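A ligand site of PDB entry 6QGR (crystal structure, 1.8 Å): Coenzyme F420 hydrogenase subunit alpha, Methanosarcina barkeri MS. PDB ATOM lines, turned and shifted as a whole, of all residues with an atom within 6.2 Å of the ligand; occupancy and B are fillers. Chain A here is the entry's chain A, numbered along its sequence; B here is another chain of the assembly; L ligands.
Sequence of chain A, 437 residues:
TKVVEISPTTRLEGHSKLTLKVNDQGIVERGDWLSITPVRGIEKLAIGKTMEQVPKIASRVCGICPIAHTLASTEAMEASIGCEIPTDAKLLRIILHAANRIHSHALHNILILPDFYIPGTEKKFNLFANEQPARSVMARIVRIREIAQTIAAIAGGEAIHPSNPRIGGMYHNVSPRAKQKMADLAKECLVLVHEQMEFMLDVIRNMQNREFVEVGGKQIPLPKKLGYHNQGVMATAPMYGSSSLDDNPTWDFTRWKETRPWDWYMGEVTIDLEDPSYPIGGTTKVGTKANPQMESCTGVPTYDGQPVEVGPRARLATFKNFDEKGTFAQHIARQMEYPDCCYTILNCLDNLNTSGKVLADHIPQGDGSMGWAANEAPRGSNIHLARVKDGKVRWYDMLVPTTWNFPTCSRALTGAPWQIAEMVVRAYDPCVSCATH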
ATOM      1  N   GLU A  13      34.174  -2.114  -1.418  1.00  0.00           N
ATOM      2  CA  GLU A  13      33.234  -3.247  -1.442  1.00  0.00           C
ATOM      3  C   GLU A  13      31.904  -2.798  -2.059  1.00  0.00           C
ATOM      4  O   GLU A  13      31.387  -1.737  -1.724  1.00  0.00           O
ATOM      5  CB  GLU A  13      32.989  -3.841  -0.054  1.00  0.00           C
ATOM      6  CG  GLU A  13      32.259  -5.169  -0.127  1.00  0.00           C
ATOM      7  CD  GLU A  13      30.760  -4.983  -0.295  1.00  0.00           C
ATOM      8  OE1 GLU A  13      30.213  -3.929   0.102  1.00  0.00           O
ATOM      9  OE2 GLU A  13      30.124  -5.871  -0.860  1.00  0.00           O
ATOM     10  N   VAL A  61      24.709  -9.907   5.254  1.00  0.00           N
ATOM     11  CA  VAL A  61      24.781  -8.583   4.673  1.00  0.00           C
ATOM     12  C   VAL A  61      26.156  -8.332   4.038  1.00  0.00           C
ATOM     13  O   VAL A  61      26.258  -7.682   2.991  1.00  0.00           O
ATOM     14  CB  VAL A  61      24.417  -7.515   5.730  1.00  0.00           C
ATOM     15  CG1 VAL A  61      24.974  -6.135   5.261  1.00  0.00           C
ATOM     16  CG2 VAL A  61      22.922  -7.460   5.952  1.00  0.00           C
ATOM     17  N   CYS A  62      27.225  -8.869   4.656  1.00  0.00           N
ATOM     18  CA  CYS A  62      28.585  -8.525   4.244  1.00  0.00           C
ATOM     19  C   CYS A  62      29.573  -9.614   4.658  1.00  0.00           C
ATOM     20  O   CYS A  62      29.598 -10.024   5.822  1.00  0.00           O
ATOM     21  CB  CYS A  62      29.037  -7.198   4.855  1.00  0.00           C
ATOM     22  SG  CYS A  62      30.790  -6.911   4.386  1.00  0.00           S
ATOM     23  N   GLY A  63      30.411 -10.043   3.697  1.00  0.00           N
ATOM     24  CA  GLY A  63      31.393 -11.080   3.960  1.00  0.00           C
ATOM     25  C   GLY A  63      32.755 -10.604   4.458  1.00  0.00           C
ATOM     26  O   GLY A  63      33.635 -11.424   4.760  1.00  0.00           O
ATOM     27  N   ILE A  64      32.964  -9.297   4.490  1.00  0.00           N
ATOM     28  CA  ILE A  64      34.179  -8.717   5.055  1.00  0.00           C
ATOM     29  C   ILE A  64      34.015  -8.463   6.545  1.00  0.00           C
ATOM     30  O   ILE A  64      34.924  -8.734   7.331  1.00  0.00           O
ATOM     31  CB  ILE A  64      34.527  -7.411   4.316  1.00  0.00           C
ATOM     32  CG1 ILE A  64      34.782  -7.671   2.832  1.00  0.00           C
ATOM     33  CG2 ILE A  64      35.758  -6.736   4.949  1.00  0.00           C
ATOM     34  CD1 ILE A  64      34.913  -6.390   2.037  1.00  0.00           C
ATOM     35  N   CYS A  65      32.868  -7.947   6.927  1.00  0.00           N
ATOM     36  CA  CYS A  65      32.579  -7.653   8.327  1.00  0.00           C
ATOM     37  C   CYS A  65      31.396  -8.477   8.880  1.00  0.00           C
ATOM     38  O   CYS A  65      30.532  -7.917   9.575  1.00  0.00           O
ATOM     39  CB  CYS A  65      32.324  -6.144   8.447  1.00  0.00           C
ATOM     40  SG  CYS A  65      30.738  -5.660   7.745  1.00  0.00           S
ATOM     41  N   PRO A  66      31.293  -9.796   8.607  1.00  0.00           N
ATOM     42  CA  PRO A  66      30.107 -10.519   9.112  1.00  0.00           C
ATOM     43  C   PRO A  66      30.101 -10.593  10.628  1.00  0.00           C
ATOM     44  O   PRO A  66      29.032 -10.650  11.244  1.00  0.00           O
ATOM     45  CB  PRO A  66      30.228 -11.899   8.440  1.00  0.00           C
ATOM     46  CG  PRO A  66      31.664 -12.111   8.249  1.00  0.00           C
ATOM     47  CD  PRO A  66      32.177 -10.706   7.854  1.00  0.00           C
ATOM     48  N   ALA A  68      30.658  -8.176  12.552  1.00  0.00           N
ATOM     49  CA  ALA A  68      29.969  -6.984  13.060  1.00  0.00           C
ATOM     50  C   ALA A  68      28.439  -7.176  13.130  1.00  0.00           C
ATOM     51  O   ALA A  68      27.807  -6.778  14.100  1.00  0.00           O
ATOM     52  CB  ALA A  68      30.290  -5.759  12.196  1.00  0.00           C
ATOM     53  N   HIS A  69      27.843  -7.737  12.071  1.00  0.00           N
ATOM     54  CA  HIS A  69      26.403  -7.909  12.057  1.00  0.00           C
ATOM     55  C   HIS A  69      25.975  -9.092  12.935  1.00  0.00           C
ATOM     56  O   HIS A  69      24.921  -9.041  13.554  1.00  0.00           O
ATOM     57  CB  HIS A  69      25.906  -8.063  10.611  1.00  0.00           C
ATOM     58  CG  HIS A  69      26.127  -6.853   9.777  1.00  0.00           C
ATOM     59  ND1 HIS A  69      25.547  -5.627  10.094  1.00  0.00           N
ATOM     60  CD2 HIS A  69      26.916  -6.632   8.696  1.00  0.00           C
ATOM     61  CE1 HIS A  69      25.934  -4.724   9.209  1.00  0.00           C
ATOM     62  NE2 HIS A  69      26.782  -5.298   8.361  1.00  0.00           N
ATOM     63  N   SER A 104      40.264  -7.138   8.173  1.00  0.00           N
ATOM     64  CA  SER A 104      39.584  -6.120   7.359  1.00  0.00           C
ATOM     65  C   SER A 104      40.525  -4.961   7.033  1.00  0.00           C
ATOM     66  O   SER A 104      40.597  -4.531   5.889  1.00  0.00           O
ATOM     67  CB  SER A 104      38.316  -5.637   8.055  1.00  0.00           C
ATOM     68  OG  SER A 104      37.597  -4.704   7.293  1.00  0.00           O
ATOM     69  N   ASN A 375      28.111  -2.339  17.695  1.00  0.00           N
ATOM     70  CA  ASN A 375      29.403  -2.966  17.477  1.00  0.00           C
ATOM     71  C   ASN A 375      30.284  -1.991  16.679  1.00  0.00           C
ATOM     72  O   ASN A 375      29.844  -1.439  15.663  1.00  0.00           O
ATOM     73  CB  ASN A 375      29.225  -4.288  16.712  1.00  0.00           C
ATOM     74  CG  ASN A 375      30.549  -4.989  16.442  1.00  0.00           C
ATOM     75  OD1 ASN A 375      31.192  -4.675  15.463  1.00  0.00           O
ATOM     76  ND2 ASN A 375      30.946  -5.937  17.307  1.00  0.00           N
ATOM     77  N   ALA A 377      32.393  -1.930  14.243  1.00  0.00           N
ATOM     78  CA  ALA A 377      32.875  -2.681  13.062  1.00  0.00           C
ATOM     79  C   ALA A 377      34.153  -2.029  12.520  1.00  0.00           C
ATOM     80  O   ALA A 377      34.463  -0.896  12.886  1.00  0.00           O
ATOM     81  CB  ALA A 377      31.802  -2.722  11.961  1.00  0.00           C
ATOM     82  N   PRO A 378      34.913  -2.702  11.664  1.00  0.00           N
ATOM     83  CA  PRO A 378      36.150  -2.052  11.171  1.00  0.00           C
ATOM     84  C   PRO A 378      35.883  -0.687  10.531  1.00  0.00           C
ATOM     85  O   PRO A 378      36.736   0.204  10.669  1.00  0.00           O
ATOM     86  CB  PRO A 378      36.699  -3.073  10.152  1.00  0.00           C
ATOM     87  CG  PRO A 378      36.140  -4.444  10.691  1.00  0.00           C
ATOM     88  CD  PRO A 378      34.764  -4.107  11.183  1.00  0.00           C
ATOM     89  N   ARG A 379      34.711  -0.491   9.909  1.00  0.00           N
ATOM     90  CA  ARG A 379      34.405   0.792   9.258  1.00  0.00           C
ATOM     91  C   ARG A 379      33.669   1.792  10.149  1.00  0.00           C
ATOM     92  O   ARG A 379      33.462   2.929   9.709  1.00  0.00           O
ATOM     93  CB  ARG A 379      33.626   0.548   7.967  1.00  0.00           C
ATOM     94  CG  ARG A 379      34.484  -0.305   7.020  1.00  0.00           C
ATOM     95  CD  ARG A 379      33.778  -1.088   5.934  1.00  0.00           C
ATOM     96  NE  ARG A 379      34.895  -1.715   5.177  1.00  0.00           N
ATOM     97  CZ  ARG A 379      35.510  -2.814   5.585  1.00  0.00           C
ATOM     98  NH1 ARG A 379      36.574  -3.288   4.949  1.00  0.00           N
ATOM     99  NH2 ARG A 379      35.036  -3.474   6.669  1.00  0.00           N
ATOM    100  N   GLY A 380      33.245   1.411  11.376  1.00  0.00           N
ATOM    101  CA  GLY A 380      32.695   2.371  12.329  1.00  0.00           C
ATOM    102  C   GLY A 380      31.465   1.798  13.050  1.00  0.00           C
ATOM    103  O   GLY A 380      31.241   0.594  13.019  1.00  0.00           O
ATOM    104  N   SER A 381      30.668   2.670  13.703  1.00  0.00           N
ATOM    105  CA  SER A 381      29.595   2.257  14.616  1.00  0.00           C
ATOM    106  C   SER A 381      28.482   1.548  13.843  1.00  0.00           C
ATOM    107  O   SER A 381      27.874   2.131  12.944  1.00  0.00           O
ATOM    108  CB  SER A 381      28.984   3.452  15.356  1.00  0.00           C
ATOM    109  OG  SER A 381      29.969   4.302  15.948  1.00  0.00           O
ATOM    110  N   ASN A 382      28.242   0.291  14.189  1.00  0.00           N
ATOM    111  CA  ASN A 382      27.204  -0.539  13.578  1.00  0.00           C
ATOM    112  C   ASN A 382      26.137  -0.790  14.654  1.00  0.00           C
ATOM    113  O   ASN A 382      26.387  -1.493  15.640  1.00  0.00           O
ATOM    114  CB  ASN A 382      27.809  -1.853  13.089  1.00  0.00           C
ATOM    115  CG  ASN A 382      26.781  -2.746  12.402  1.00  0.00           C
ATOM    116  OD1 ASN A 382      25.882  -2.265  11.725  1.00  0.00           O
ATOM    117  ND2 ASN A 382      26.902  -4.046  12.602  1.00  0.00           N
ATOM    118  N   HIS A 384      22.392  -1.954  15.703  1.00  0.00           N
ATOM    119  CA  HIS A 384      21.204  -2.753  15.460  1.00  0.00           C
ATOM    120  C   HIS A 384      20.209  -2.519  16.623  1.00  0.00           C
ATOM    121  O   HIS A 384      20.611  -2.525  17.808  1.00  0.00           O
ATOM    122  CB  HIS A 384      21.538  -4.250  15.382  1.00  0.00           C
ATOM    123  CG  HIS A 384      22.273  -4.639  14.134  1.00  0.00           C
ATOM    124  ND1 HIS A 384      22.001  -5.805  13.447  1.00  0.00           N
ATOM    125  CD2 HIS A 384      23.241  -4.004  13.425  1.00  0.00           C
ATOM    126  CE1 HIS A 384      22.791  -5.889  12.398  1.00  0.00           C
ATOM    127  NE2 HIS A 384      23.569  -4.815  12.368  1.00  0.00           N
ATOM    128  N   VAL A 400      24.269   1.152   9.773  1.00  0.00           N
ATOM    129  CA  VAL A 400      25.537   0.493   9.458  1.00  0.00           C
ATOM    130  C   VAL A 400      26.593   1.556   9.102  1.00  0.00           C
ATOM    131  O   VAL A 400      26.259   2.607   8.535  1.00  0.00           O
ATOM    132  CB  VAL A 400      25.324  -0.555   8.346  1.00  0.00           C
ATOM    133  CG1 VAL A 400      26.557  -1.469   8.068  1.00  0.00           C
ATOM    134  CG2 VAL A 400      24.121  -1.435   8.675  1.00  0.00           C
ATOM    135  N   PRO A 401      27.884   1.326   9.438  1.00  0.00           N
ATOM    136  CA  PRO A 401      28.860   2.436   9.325  1.00  0.00           C
ATOM    137  C   PRO A 401      28.849   3.119   7.971  1.00  0.00           C
ATOM    138  O   PRO A 401      28.836   4.358   7.908  1.00  0.00           O
ATOM    139  CB  PRO A 401      30.208   1.737   9.607  1.00  0.00           C
ATOM    140  CG  PRO A 401      29.842   0.223   9.956  1.00  0.00           C
ATOM    141  CD  PRO A 401      28.404   0.228  10.267  1.00  0.00           C
ATOM    142  N   THR A 402      28.901   2.332   6.873  1.00  0.00           N
ATOM    143  CA  THR A 402      28.994   2.990   5.563  1.00  0.00           C
ATOM    144  C   THR A 402      27.691   3.731   5.261  1.00  0.00           C
ATOM    145  O   THR A 402      27.724   4.763   4.593  1.00  0.00           O
ATOM    146  CB  THR A 402      29.403   1.966   4.454  1.00  0.00           C
ATOM    147  OG1 THR A 402      30.713   1.468   4.720  1.00  0.00           O
ATOM    148  CG2 THR A 402      29.518   2.616   3.064  1.00  0.00           C
ATOM    149  N   THR A 403      26.548   3.272   5.788  1.00  0.00           N
ATOM    150  CA  THR A 403      25.333   4.083   5.690  1.00  0.00           C
ATOM    151  C   THR A 403      25.563   5.492   6.256  1.00  0.00           C
ATOM    152  O   THR A 403      25.174   6.502   5.645  1.00  0.00           O
ATOM    153  CB  THR A 403      24.156   3.422   6.448  1.00  0.00           C
ATOM    154  OG1 THR A 403      24.169   1.982   6.318  1.00  0.00           O
ATOM    155  CG2 THR A 403      22.823   3.960   5.962  1.00  0.00           C
ATOM    156  N   ASP A 429      37.025   3.496   3.507  1.00  0.00           N
ATOM    157  CA  ASP A 429      37.009   2.034   3.465  1.00  0.00           C
ATOM    158  C   ASP A 429      35.565   1.550   3.236  1.00  0.00           C
ATOM    159  O   ASP A 429      35.016   0.800   4.040  1.00  0.00           O
ATOM    160  CB  ASP A 429      37.607   1.491   4.767  1.00  0.00           C
ATOM    161  CG  ASP A 429      37.726  -0.069   4.831  1.00  0.00           C
ATOM    162  OD1 ASP A 429      37.481  -0.758   3.815  1.00  0.00           O
ATOM    163  OD2 ASP A 429      38.091  -0.592   5.950  1.00  0.00           O
ATOM    164  N   PRO A 430      34.907   2.001   2.154  1.00  0.00           N
ATOM    165  CA  PRO A 430      33.456   1.773   2.020  1.00  0.00           C
ATOM    166  C   PRO A 430      33.080   0.302   1.899  1.00  0.00           C
ATOM    167  O   PRO A 430      33.764  -0.486   1.227  1.00  0.00           O
ATOM    168  CB  PRO A 430      33.092   2.525   0.712  1.00  0.00           C
ATOM    169  CG  PRO A 430      34.122   3.601   0.601  1.00  0.00           C
ATOM    170  CD  PRO A 430      35.402   2.874   1.074  1.00  0.00           C
ATOM    171  N   CYS A 431      31.950  -0.042   2.530  1.00  0.00           N
ATOM    172  CA  CYS A 431      31.296  -1.331   2.335  1.00  0.00           C
ATOM    173  C   CYS A 431      29.848  -1.062   1.918  1.00  0.00           C
ATOM    174  O   CYS A 431      28.954  -0.803   2.747  1.00  0.00           O
ATOM    175  CB  CYS A 431      31.403  -2.189   3.617  1.00  0.00           C
ATOM    176  SG  CYS A 431      30.927  -3.863   3.236  1.00  0.00           S
ATOM    177  N   VAL A 432      29.612  -1.078   0.612  1.00  0.00           N
ATOM    178  CA  VAL A 432      28.318  -0.601   0.114  1.00  0.00           C
ATOM    179  C   VAL A 432      27.213  -1.658   0.289  1.00  0.00           C
ATOM    180  O   VAL A 432      26.050  -1.306   0.508  1.00  0.00           O
ATOM    181  CB  VAL A 432      28.456  -0.105  -1.346  1.00  0.00           C
ATOM    182  CG1 VAL A 432      27.084   0.428  -1.905  1.00  0.00           C
ATOM    183  CG2 VAL A 432      29.497   1.033  -1.391  1.00  0.00           C
ATOM    184  N   SER A 433      27.557  -2.948   0.269  1.00  0.00           N
ATOM    185  CA  SER A 433      26.587  -3.972   0.681  1.00  0.00           C
ATOM    186  C   SER A 433      26.150  -3.784   2.145  1.00  0.00           C
ATOM    187  O   SER A 433      24.940  -3.819   2.426  1.00  0.00           O
ATOM    188  CB  SER A 433      27.149  -5.362   0.460  1.00  0.00           C
ATOM    189  OG  SER A 433      27.407  -5.579  -0.911  1.00  0.00           O
ATOM    190  N   CYS A 434      27.101  -3.506   3.071  1.00  0.00           N
ATOM    191  CA  CYS A 434      26.744  -3.084   4.432  1.00  0.00           C
ATOM    192  C   CYS A 434      25.816  -1.881   4.468  1.00  0.00           C
ATOM    193  O   CYS A 434      24.799  -1.886   5.166  1.00  0.00           O
ATOM    194  CB  CYS A 434      27.995  -2.708   5.222  1.00  0.00           C
ATOM    195  SG  CYS A 434      28.588  -4.110   6.055  1.00  0.00           S
ATOM    196  N   ALA A 435      26.167  -0.809   3.752  1.00  0.00           N
ATOM    197  CA  ALA A 435      25.406   0.420   3.872  1.00  0.00           C
ATOM    198  C   ALA A 435      23.943   0.226   3.458  1.00  0.00           C
ATOM    199  O   ALA A 435      23.060   0.935   3.945  1.00  0.00           O
ATOM    200  CB  ALA A 435      26.049   1.512   3.010  1.00  0.00           C
ATOM    201  N   CYS B  14      27.534 -10.622  -1.003  1.00  0.00           N
ATOM    202  CA  CYS B  14      28.065  -9.968   0.193  1.00  0.00           C
ATOM    203  C   CYS B  14      29.580  -9.751   0.146  1.00  0.00           C
ATOM    204  O   CYS B  14      30.138  -9.121   1.059  1.00  0.00           O
ATOM    205  CB  CYS B  14      27.641 -10.779   1.456  1.00  0.00           C
ATOM    206  SG  CYS B  14      28.809 -12.072   1.872  1.00  0.00           S
HETATM  207 FE1  LIG L   1      30.437  -3.297   7.501  1.00  0.00          FE
HETATM  208 NI1  LIG L   1      30.976  -4.874   5.378  1.00  0.00          NI
HETATM  209  C1  LIG L   1      32.040  -2.910   8.305  1.00  0.00           C
HETATM  210  N1  LIG L   1      33.097  -2.707   8.800  1.00  0.00           N
HETATM  211  C2  LIG L   1      30.214  -1.536   7.013  1.00  0.00           C
HETATM  212  N2  LIG L   1      30.053  -0.447   6.682  1.00  0.00           N
HETATM  213  C3  LIG L   1      29.512  -3.163   9.122  1.00  0.00           C
HETATM  214  O1  LIG L   1      28.947  -3.107  10.148  1.00  0.00           O
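The backbone NH (N) of Arg 379 sits at hydrogen-bond distance from a nitrogen (N1) of the ligand (3.0 Å).
OG1 of Thr 402 sits at hydrogen-bond distance from N2 of the ligand, at 2.8 Å.
The side-chain sulfur of Cys 62 is bound to a nickel atom (NI1) of the ligand (2.3 Å).
The side-chain amide nitrogen (ND2) of Asn 382 sits close to an oxygen (O1) of the ligand (3.3 Å).
NH2 of Arg 379 lies within hydrogen-bond range of N1 of the ligand, at 3.0 Å.
SG of Cys 65 is bound to FE1 of the ligand.
The side-chain sulfur (SG) of Cys 431 binds a nickel atom (NI1) of the ligand, at 2.4 Å.
The side-chain sulfur (SG) of Cys 434 binds an iron atom (FE1) of the ligand.
The backbone NH of Thr 402 is in hydrogen-bond range of a nitrogen (N2) of the ligand (3.0 Å).
NH2 of Arg 379 lies within hydrogen-bond range of OG of Ser 104, 2.9 Å away.
The side-chain sulfur (SG) of Cys 434 sits close to a ring nitrogen (NE2) of His 69, 3.2 Å away.
OG1 of Thr 403 sits close to O of Val 400 (3.1 Å).
The backbone NH (N) of Cys 431 lies within hydrogen-bond range of the side-chain hydroxyl (OG1) of Thr 402 (2.9 Å).
N of Ile 64 lies close to SG of Cys 62 (3.2 Å).
The backbone NH of Ala 377 lies close to the side-chain amide oxygen of Asn 375 (3.2 Å).
The side-chain amide nitrogen (ND2) of Asn 382 sits at hydrogen-bond distance from a ring nitrogen (ND1) of His 69.
The guanidinium group of Arg 379 is in salt-bridge range of the side-chain carboxylate of Asp 429, at 2.9 Å.
The backbone nitrogen (N) of Pro 378 lies close to a nitrogen (N1) of the ligand (3.4 Å).
Merely in contact with the ligand: Pro 401 (3.3 Å), Ala 377 (3.4 Å), His 69 (3.5 Å), Val 400 (3.6 Å) and Ala 68 (3.6 Å).
Hydrophobic or aromatic side chains within 4 Å of the ligand: Ala 68, His 69, Ala 377, Pro 378, Val 400 and Pro 401.
Within 4 Å of the ligand: Cys 62, Cys 65, Ala 68, His 69, Ala 377, Pro 378, Arg 379, Asn 382, Val 400, Pro 401, Thr 402, Cys 431 and Cys 434.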
